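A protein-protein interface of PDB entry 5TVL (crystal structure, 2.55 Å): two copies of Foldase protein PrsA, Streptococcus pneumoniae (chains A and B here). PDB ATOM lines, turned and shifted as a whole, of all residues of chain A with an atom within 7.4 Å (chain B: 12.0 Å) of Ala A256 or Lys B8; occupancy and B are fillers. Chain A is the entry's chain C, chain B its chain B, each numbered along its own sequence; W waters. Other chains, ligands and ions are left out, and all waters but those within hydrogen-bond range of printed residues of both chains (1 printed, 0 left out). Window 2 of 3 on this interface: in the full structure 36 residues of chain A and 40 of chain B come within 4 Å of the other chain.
Of the printed residues of chain B, Thr A35 touches Ile B5 (3.6 Å) and Ile B12 (3.2 Å). No residue of chain B comes within 4 Å of Val A39. Leu A253 touches none of the printed residues of chain B. Ala A256 touches just these residues of chain B: Met B7 and Lys B8. Ile A258 touches just these residues of chain B: Ser B6 (3.2 Å) and Met B7 (3.9 Å). Of the printed residues of chain B, Lys A259 touches Leu B4 (3.98 Å), Ile B5 (3.5 Å) and Ser B6 (2.9 Å). Printed residues of chain A within 4 Å of Lys B8: Ala A256 (3.1 Å). Gly B9 touches none of the printed residues of chain A. The nearest residue of chain B that does not touch Ala A256 is Ser B6 (5.4 Å).
Among the printed residues, merely in contact across the chains: Thr A35 with Ile B5 (3.6 Å), Thr A35 with Ile B12 (3.2 Å), Lys A38 with Val B11 (3.6 Å), Lys A38 with Ile B12 (3.7 Å), Ala A256 with Met B7 (3.6 Å), Asn A257 with Ser B6 (3.7 Å), Asn A257 with Met B7 (3.9 Å), Ile A258 with Ser B6 (3.2 Å), Ile A258 with Met B7 (3.9 Å), Lys A259 with Leu B4 (3.98 Å) and Lys A259 with Ile B5 (3.5 Å).
The backbone NH of Leu B4 lies within hydrogen-bond range of the backbone carbonyl oxygen of Ile B12 (2.9 Å). N of Ile B12 lies within hydrogen-bond range of O of Ile B5 (2.8 Å).
No position is printed for both chains. Of the 14 pairs that touch across the chains among the printed residues, none has its exchanged pair printed and touching as well.
Of the 10 printed residues of chain B, 8 touch a printed residue of chain A. Of the 16 printed residues of chain A, 6 touch a printed residue of chain B. Hydrophobic or aromatic side chains of chain A within 4 Å of the printed part of chain B: Ile A258.
Water W1 lies within hydrogen-bond range of O of Lys A38 (3.4 Å) and SD of Met B7 (3.5 Å).
The backbone carbonyl oxygen (O) of Ser B6 sits at hydrogen-bond distance from the backbone NH (N) of Lys A259, at 2.9 Å. The backbone carbonyl oxygen (O) of Ala A256 lies within hydrogen-bond range of the backbone NH (N) of Lys B8. The side-chain carboxylate (OD1) of Asp B10 is in salt-bridge range of the side-chain amino group (NZ) of Lys A38 (3.7 Å).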
ATOM      1  N   THR A  35     -17.022 -10.798 -10.495  1.00  0.00           N
ATOM      2  CA  THR A  35     -16.879  -9.439 -11.034  1.00  0.00           C
ATOM      3  C   THR A  35     -15.812  -9.334 -12.132  1.00  0.00           C
ATOM      4  O   THR A  35     -15.995  -8.602 -13.107  1.00  0.00           O
ATOM      5  CB  THR A  35     -16.556  -8.421  -9.915  1.00  0.00           C
ATOM      6  OG1 THR A  35     -17.478  -8.589  -8.826  1.00  0.00           O
ATOM      7  CG2 THR A  35     -16.653  -6.981 -10.438  1.00  0.00           C
ATOM      8  N   LYS A  38     -17.514 -11.073 -15.240  1.00  0.00           N
ATOM      9  CA  LYS A  38     -18.513 -10.238 -15.937  1.00  0.00           C
ATOM     10  C   LYS A  38     -17.882  -9.103 -16.744  1.00  0.00           C
ATOM     11  O   LYS A  38     -18.243  -8.895 -17.905  1.00  0.00           O
ATOM     12  CB  LYS A  38     -19.558  -9.654 -14.970  1.00  0.00           C
ATOM     13  CG  LYS A  38     -20.800 -10.511 -14.780  1.00  0.00           C
ATOM     14  CD  LYS A  38     -21.881  -9.726 -14.052  1.00  0.00           C
ATOM     15  CE  LYS A  38     -23.032 -10.614 -13.592  1.00  0.00           C
ATOM     16  NZ  LYS A  38     -23.932 -11.034 -14.703  1.00  0.00           N
ATOM     17  N   VAL A  39     -16.946  -8.392 -16.117  1.00  0.00           N
ATOM     18  CA  VAL A  39     -16.247  -7.261 -16.740  1.00  0.00           C
ATOM     19  C   VAL A  39     -15.462  -7.713 -17.978  1.00  0.00           C
ATOM     20  O   VAL A  39     -15.594  -7.112 -19.050  1.00  0.00           O
ATOM     21  CB  VAL A  39     -15.324  -6.540 -15.720  1.00  0.00           C
ATOM     22  CG1 VAL A  39     -14.363  -5.561 -16.398  1.00  0.00           C
ATOM     23  CG2 VAL A  39     -16.170  -5.815 -14.681  1.00  0.00           C
ATOM     24  N   PHE A  40     -14.668  -8.771 -17.824  1.00  0.00           N
ATOM     25  CA  PHE A  40     -13.898  -9.338 -18.940  1.00  0.00           C
ATOM     26  C   PHE A  40     -14.772 -10.051 -19.978  1.00  0.00           C
ATOM     27  O   PHE A  40     -14.401 -10.111 -21.149  1.00  0.00           O
ATOM     28  CB  PHE A  40     -12.786 -10.275 -18.435  1.00  0.00           C
ATOM     29  CG  PHE A  40     -11.536  -9.552 -18.016  1.00  0.00           C
ATOM     30  CD1 PHE A  40     -11.428  -8.972 -16.755  1.00  0.00           C
ATOM     31  CD2 PHE A  40     -10.464  -9.434 -18.893  1.00  0.00           C
ATOM     32  CE1 PHE A  40     -10.273  -8.294 -16.378  1.00  0.00           C
ATOM     33  CE2 PHE A  40      -9.309  -8.760 -18.518  1.00  0.00           C
ATOM     34  CZ  PHE A  40      -9.211  -8.193 -17.264  1.00  0.00           C
ATOM     35  N   LYS A  42     -17.805  -8.935 -20.847  1.00  0.00           N
ATOM     36  CA  LYS A  42     -18.332  -7.797 -21.605  1.00  0.00           C
ATOM     37  C   LYS A  42     -17.283  -7.253 -22.582  1.00  0.00           C
ATOM     38  O   LYS A  42     -17.601  -6.975 -23.741  1.00  0.00           O
ATOM     39  CB  LYS A  42     -18.812  -6.692 -20.645  1.00  0.00           C
ATOM     40  CG  LYS A  42     -19.322  -5.408 -21.293  1.00  0.00           C
ATOM     41  CD  LYS A  42     -20.581  -5.624 -22.118  1.00  0.00           C
ATOM     42  CE  LYS A  42     -20.978  -4.357 -22.864  1.00  0.00           C
ATOM     43  NZ  LYS A  42     -21.270  -3.210 -21.959  1.00  0.00           N
ATOM     44  N   GLN A  43     -16.041  -7.130 -22.112  1.00  0.00           N
ATOM     45  CA  GLN A  43     -14.970  -6.508 -22.885  1.00  0.00           C
ATOM     46  C   GLN A  43     -14.438  -7.400 -24.001  1.00  0.00           C
ATOM     47  O   GLN A  43     -14.380  -6.968 -25.153  1.00  0.00           O
ATOM     48  CB  GLN A  43     -13.816  -6.097 -21.962  1.00  0.00           C
ATOM     49  CG  GLN A  43     -12.786  -5.163 -22.599  1.00  0.00           C
ATOM     50  CD  GLN A  43     -13.248  -3.714 -22.697  1.00  0.00           C
ATOM     51  OE1 GLN A  43     -14.443  -3.420 -22.676  1.00  0.00           O
ATOM     52  NE2 GLN A  43     -12.292  -2.799 -22.800  1.00  0.00           N
ATOM     53  N   GLY A 250      -7.048  -4.556 -13.073  1.00  0.00           N
ATOM     54  CA  GLY A 250      -7.393  -3.285 -12.421  1.00  0.00           C
ATOM     55  C   GLY A 250      -7.956  -2.230 -13.361  1.00  0.00           C
ATOM     56  O   GLY A 250      -8.971  -1.602 -13.061  1.00  0.00           O
ATOM     57  N   LYS A 251      -7.305  -2.051 -14.509  1.00  0.00           N
ATOM     58  CA  LYS A 251      -7.732  -1.051 -15.496  1.00  0.00           C
ATOM     59  C   LYS A 251      -9.034  -1.416 -16.193  1.00  0.00           C
ATOM     60  O   LYS A 251      -9.836  -0.528 -16.486  1.00  0.00           O
ATOM     61  CB  LYS A 251      -6.628  -0.786 -16.523  1.00  0.00           C
ATOM     62  CG  LYS A 251      -5.416  -0.073 -15.939  1.00  0.00           C
ATOM     63  CD  LYS A 251      -5.683   1.403 -15.662  1.00  0.00           C
ATOM     64  CE  LYS A 251      -4.664   1.968 -14.687  1.00  0.00           C
ATOM     65  NZ  LYS A 251      -4.886   3.413 -14.410  1.00  0.00           N
ATOM     66  N   GLU A 252      -9.252  -2.708 -16.445  1.00  0.00           N
ATOM     67  CA  GLU A 252     -10.517  -3.172 -17.036  1.00  0.00           C
ATOM     68  C   GLU A 252     -11.694  -3.003 -16.067  1.00  0.00           C
ATOM     69  O   GLU A 252     -12.815  -2.709 -16.504  1.00  0.00           O
ATOM     70  CB  GLU A 252     -10.425  -4.632 -17.507  1.00  0.00           C
ATOM     71  CG  GLU A 252     -10.995  -4.865 -18.894  1.00  0.00           C
ATOM     72  CD  GLU A 252     -10.169  -4.194 -19.978  1.00  0.00           C
ATOM     73  OE1 GLU A 252     -10.709  -3.295 -20.652  1.00  0.00           O
ATOM     74  OE2 GLU A 252      -8.977  -4.544 -20.134  1.00  0.00           O
ATOM     75  N   LEU A 253     -11.433  -3.186 -14.767  1.00  0.00           N
ATOM     76  CA  LEU A 253     -12.446  -2.990 -13.717  1.00  0.00           C
ATOM     77  C   LEU A 253     -12.786  -1.508 -13.537  1.00  0.00           C
ATOM     78  O   LEU A 253     -13.964  -1.147 -13.437  1.00  0.00           O
ATOM     79  CB  LEU A 253     -11.991  -3.602 -12.379  1.00  0.00           C
ATOM     80  CG  LEU A 253     -11.875  -5.134 -12.301  1.00  0.00           C
ATOM     81  CD1 LEU A 253     -11.272  -5.562 -10.970  1.00  0.00           C
ATOM     82  CD2 LEU A 253     -13.222  -5.809 -12.521  1.00  0.00           C
ATOM     83  N   GLN A 254     -11.755  -0.660 -13.511  1.00  0.00           N
ATOM     84  CA  GLN A 254     -11.934   0.806 -13.473  1.00  0.00           C
ATOM     85  C   GLN A 254     -12.709   1.344 -14.686  1.00  0.00           C
ATOM     86  O   GLN A 254     -13.521   2.259 -14.553  1.00  0.00           O
ATOM     87  CB  GLN A 254     -10.578   1.513 -13.381  1.00  0.00           C
ATOM     88  CG  GLN A 254      -9.850   1.310 -12.058  1.00  0.00           C
ATOM     89  CD  GLN A 254      -8.345   1.523 -12.177  1.00  0.00           C
ATOM     90  OE1 GLN A 254      -7.892   2.516 -12.745  1.00  0.00           O
ATOM     91  NE2 GLN A 254      -7.566   0.589 -11.642  1.00  0.00           N
ATOM     92  N   ALA A 255     -12.452   0.770 -15.859  1.00  0.00           N
ATOM     93  CA  ALA A 255     -13.183   1.116 -17.086  1.00  0.00           C
ATOM     94  C   ALA A 255     -14.636   0.614 -17.094  1.00  0.00           C
ATOM     95  O   ALA A 255     -15.488   1.202 -17.760  1.00  0.00           O
ATOM     96  CB  ALA A 255     -12.445   0.590 -18.310  1.00  0.00           C
ATOM     97  N   ALA A 256     -14.908  -0.480 -16.383  1.00  0.00           N
ATOM     98  CA  ALA A 256     -16.277  -0.967 -16.185  1.00  0.00           C
ATOM     99  C   ALA A 256     -17.058  -0.159 -15.133  1.00  0.00           C
ATOM    100  O   ALA A 256     -18.287  -0.260 -15.076  1.00  0.00           O
ATOM    101  CB  ALA A 256     -16.262  -2.440 -15.807  1.00  0.00           C
ATOM    102  N   ASN A 257     -16.346   0.610 -14.302  1.00  0.00           N
ATOM    103  CA  ASN A 257     -16.941   1.485 -13.281  1.00  0.00           C
ATOM    104  C   ASN A 257     -17.754   0.676 -12.264  1.00  0.00           C
ATOM    105  O   ASN A 257     -18.954   0.904 -12.072  1.00  0.00           O
ATOM    106  CB  ASN A 257     -17.783   2.600 -13.929  1.00  0.00           C
ATOM    107  CG  ASN A 257     -18.241   3.657 -12.927  1.00  0.00           C
ATOM    108  OD1 ASN A 257     -17.495   4.049 -12.029  1.00  0.00           O
ATOM    109  ND2 ASN A 257     -19.477   4.129 -13.087  1.00  0.00           N
ATOM    110  N   ILE A 258     -17.089  -0.285 -11.625  1.00  0.00           N
ATOM    111  CA  ILE A 258     -17.757  -1.146 -10.642  1.00  0.00           C
ATOM    112  C   ILE A 258     -18.007  -0.392  -9.336  1.00  0.00           C
ATOM    113  O   ILE A 258     -17.110   0.268  -8.813  1.00  0.00           O
ATOM    114  CB  ILE A 258     -17.023  -2.490 -10.359  1.00  0.00           C
ATOM    115  CG1 ILE A 258     -15.524  -2.298 -10.100  1.00  0.00           C
ATOM    116  CG2 ILE A 258     -17.241  -3.463 -11.511  1.00  0.00           C
ATOM    117  CD1 ILE A 258     -14.897  -3.437  -9.332  1.00  0.00           C
ATOM    118  N   LYS A 259     -19.243  -0.472  -8.844  1.00  0.00           N
ATOM    119  CA  LYS A 259     -19.609   0.049  -7.528  1.00  0.00           C
ATOM    120  C   LYS A 259     -19.896  -1.137  -6.616  1.00  0.00           C
ATOM    121  O   LYS A 259     -20.675  -2.024  -6.974  1.00  0.00           O
ATOM    122  CB  LYS A 259     -20.848   0.941  -7.616  1.00  0.00           C
ATOM    123  CG  LYS A 259     -20.723   2.113  -8.579  1.00  0.00           C
ATOM    124  CD  LYS A 259     -22.029   2.891  -8.668  1.00  0.00           C
ATOM    125  CE  LYS A 259     -22.073   3.798  -9.888  1.00  0.00           C
ATOM    126  NZ  LYS A 259     -23.441   4.336 -10.123  1.00  0.00           N
ATOM    127  N   ASP B   3     -28.772  -5.903  -4.976  1.00  0.00           N
ATOM    128  CA  ASP B   3     -27.592  -5.985  -5.834  1.00  0.00           C
ATOM    129  C   ASP B   3     -26.339  -5.796  -4.992  1.00  0.00           C
ATOM    130  O   ASP B   3     -26.347  -5.022  -4.037  1.00  0.00           O
ATOM    131  CB  ASP B   3     -27.661  -4.920  -6.929  1.00  0.00           C
ATOM    132  CG  ASP B   3     -28.831  -5.133  -7.886  1.00  0.00           C
ATOM    133  OD1 ASP B   3     -29.465  -6.213  -7.843  1.00  0.00           O
ATOM    134  OD2 ASP B   3     -29.114  -4.214  -8.686  1.00  0.00           O
ATOM    135  N   LEU B   4     -25.283  -6.528  -5.346  1.00  0.00           N
ATOM    136  CA  LEU B   4     -24.010  -6.510  -4.619  1.00  0.00           C
ATOM    137  C   LEU B   4     -22.941  -5.722  -5.367  1.00  0.00           C
ATOM    138  O   LEU B   4     -22.192  -4.952  -4.754  1.00  0.00           O
ATOM    139  CB  LEU B   4     -23.523  -7.942  -4.382  1.00  0.00           C
ATOM    140  CG  LEU B   4     -24.502  -8.908  -3.702  1.00  0.00           C
ATOM    141  CD1 LEU B   4     -23.821 -10.241  -3.404  1.00  0.00           C
ATOM    142  CD2 LEU B   4     -25.084  -8.299  -2.430  1.00  0.00           C
ATOM    143  N   ILE B   5     -22.859  -5.941  -6.680  1.00  0.00           N
ATOM    144  CA  ILE B   5     -21.980  -5.180  -7.566  1.00  0.00           C
ATOM    145  C   ILE B   5     -22.812  -4.634  -8.722  1.00  0.00           C
ATOM    146  O   ILE B   5     -23.671  -5.337  -9.259  1.00  0.00           O
ATOM    147  CB  ILE B   5     -20.851  -6.069  -8.149  1.00  0.00           C
ATOM    148  CG1 ILE B   5     -20.052  -6.769  -7.034  1.00  0.00           C
ATOM    149  CG2 ILE B   5     -19.915  -5.258  -9.039  1.00  0.00           C
ATOM    150  CD1 ILE B   5     -19.219  -5.855  -6.157  1.00  0.00           C
ATOM    151  N   SER B   6     -22.560  -3.382  -9.094  1.00  0.00           N
ATOM    152  CA  SER B   6     -23.099  -2.806 -10.336  1.00  0.00           C
ATOM    153  C   SER B   6     -21.947  -2.319 -11.205  1.00  0.00           C
ATOM    154  O   SER B   6     -20.894  -1.933 -10.696  1.00  0.00           O
ATOM    155  CB  SER B   6     -24.070  -1.657 -10.047  1.00  0.00           C
ATOM    156  OG  SER B   6     -23.395  -0.532  -9.518  1.00  0.00           O
ATOM    157  N   MET B   7     -22.169  -2.350 -12.515  1.00  0.00           N
ATOM    158  CA  MET B   7     -21.189  -1.903 -13.510  1.00  0.00           C
ATOM    159  C   MET B   7     -21.947  -1.344 -14.722  1.00  0.00           C
ATOM    160  O   MET B   7     -23.171  -1.209 -14.670  1.00  0.00           O
ATOM    161  CB  MET B   7     -20.274  -3.075 -13.890  1.00  0.00           C
ATOM    162  CG  MET B   7     -20.977  -4.249 -14.568  1.00  0.00           C
ATOM    163  SD  MET B   7     -20.436  -5.869 -13.982  1.00  0.00           S
ATOM    164  CE  MET B   7     -21.350  -5.989 -12.451  1.00  0.00           C
ATOM    165  N   LYS B   8     -21.231  -1.000 -15.794  1.00  0.00           N
ATOM    166  CA  LYS B   8     -21.873  -0.499 -17.015  1.00  0.00           C
ATOM    167  C   LYS B   8     -22.855  -1.517 -17.605  1.00  0.00           C
ATOM    168  O   LYS B   8     -22.447  -2.527 -18.181  1.00  0.00           O
ATOM    169  CB  LYS B   8     -20.832  -0.107 -18.075  1.00  0.00           C
ATOM    170  CG  LYS B   8     -20.130   1.214 -17.802  1.00  0.00           C
ATOM    171  CD  LYS B   8     -19.481   1.775 -19.061  1.00  0.00           C
ATOM    172  CE  LYS B   8     -19.072   3.227 -18.885  1.00  0.00           C
ATOM    173  NZ  LYS B   8     -18.768   3.864 -20.196  1.00  0.00           N
ATOM    174  N   GLY B   9     -24.148  -1.240 -17.436  1.00  0.00           N
ATOM    175  CA  GLY B   9     -25.213  -2.062 -18.010  1.00  0.00           C
ATOM    176  C   GLY B   9     -25.358  -3.464 -17.440  1.00  0.00           C
ATOM    177  O   GLY B   9     -25.849  -4.361 -18.132  1.00  0.00           O
ATOM    178  N   ASP B  10     -24.937  -3.663 -16.190  1.00  0.00           N
ATOM    179  CA  ASP B  10     -25.086  -4.965 -15.530  1.00  0.00           C
ATOM    180  C   ASP B  10     -24.933  -4.879 -14.009  1.00  0.00           C
ATOM    181  O   ASP B  10     -24.346  -3.929 -13.480  1.00  0.00           O
ATOM    182  CB  ASP B  10     -24.076  -5.980 -16.098  1.00  0.00           C
ATOM    183  CG  ASP B  10     -24.630  -7.398 -16.151  1.00  0.00           C
ATOM    184  OD1 ASP B  10     -25.478  -7.756 -15.307  1.00  0.00           O
ATOM    185  OD2 ASP B  10     -24.212  -8.157 -17.049  1.00  0.00           O
ATOM    186  N   VAL B  11     -25.486  -5.879 -13.323  1.00  0.00           N
ATOM    187  CA  VAL B  11     -25.295  -6.058 -11.880  1.00  0.00           C
ATOM    188  C   VAL B  11     -25.022  -7.523 -11.562  1.00  0.00           C
ATOM    189  O   VAL B  11     -25.492  -8.414 -12.279  1.00  0.00           O
ATOM    190  CB  VAL B  11     -26.525  -5.590 -11.051  1.00  0.00           C
ATOM    191  CG1 VAL B  11     -26.595  -4.070 -10.997  1.00  0.00           C
ATOM    192  CG2 VAL B  11     -27.832  -6.175 -11.588  1.00  0.00           C
ATOM    193  N   ILE B  12     -24.238  -7.762 -10.509  1.00  0.00           N
ATOM    194  CA  ILE B  12     -24.204  -9.064  -9.834  1.00  0.00           C
ATOM    195  C   ILE B  12     -25.208  -8.963  -8.694  1.00  0.00           C
ATOM    196  O   ILE B  12     -25.042  -8.135  -7.794  1.00  0.00           O
ATOM    197  CB  ILE B  12     -22.815  -9.413  -9.254  1.00  0.00           C
ATOM    198  CG1 ILE B  12     -21.760  -9.448 -10.363  1.00  0.00           C
ATOM    199  CG2 ILE B  12     -22.855 -10.773  -8.557  1.00  0.00           C
ATOM    200  CD1 ILE B  12     -20.341  -9.660  -9.873  1.00  0.00           C
HETATM  201  O   HOH W   1     -19.895  -5.932 -17.483  1.00  0.00           O
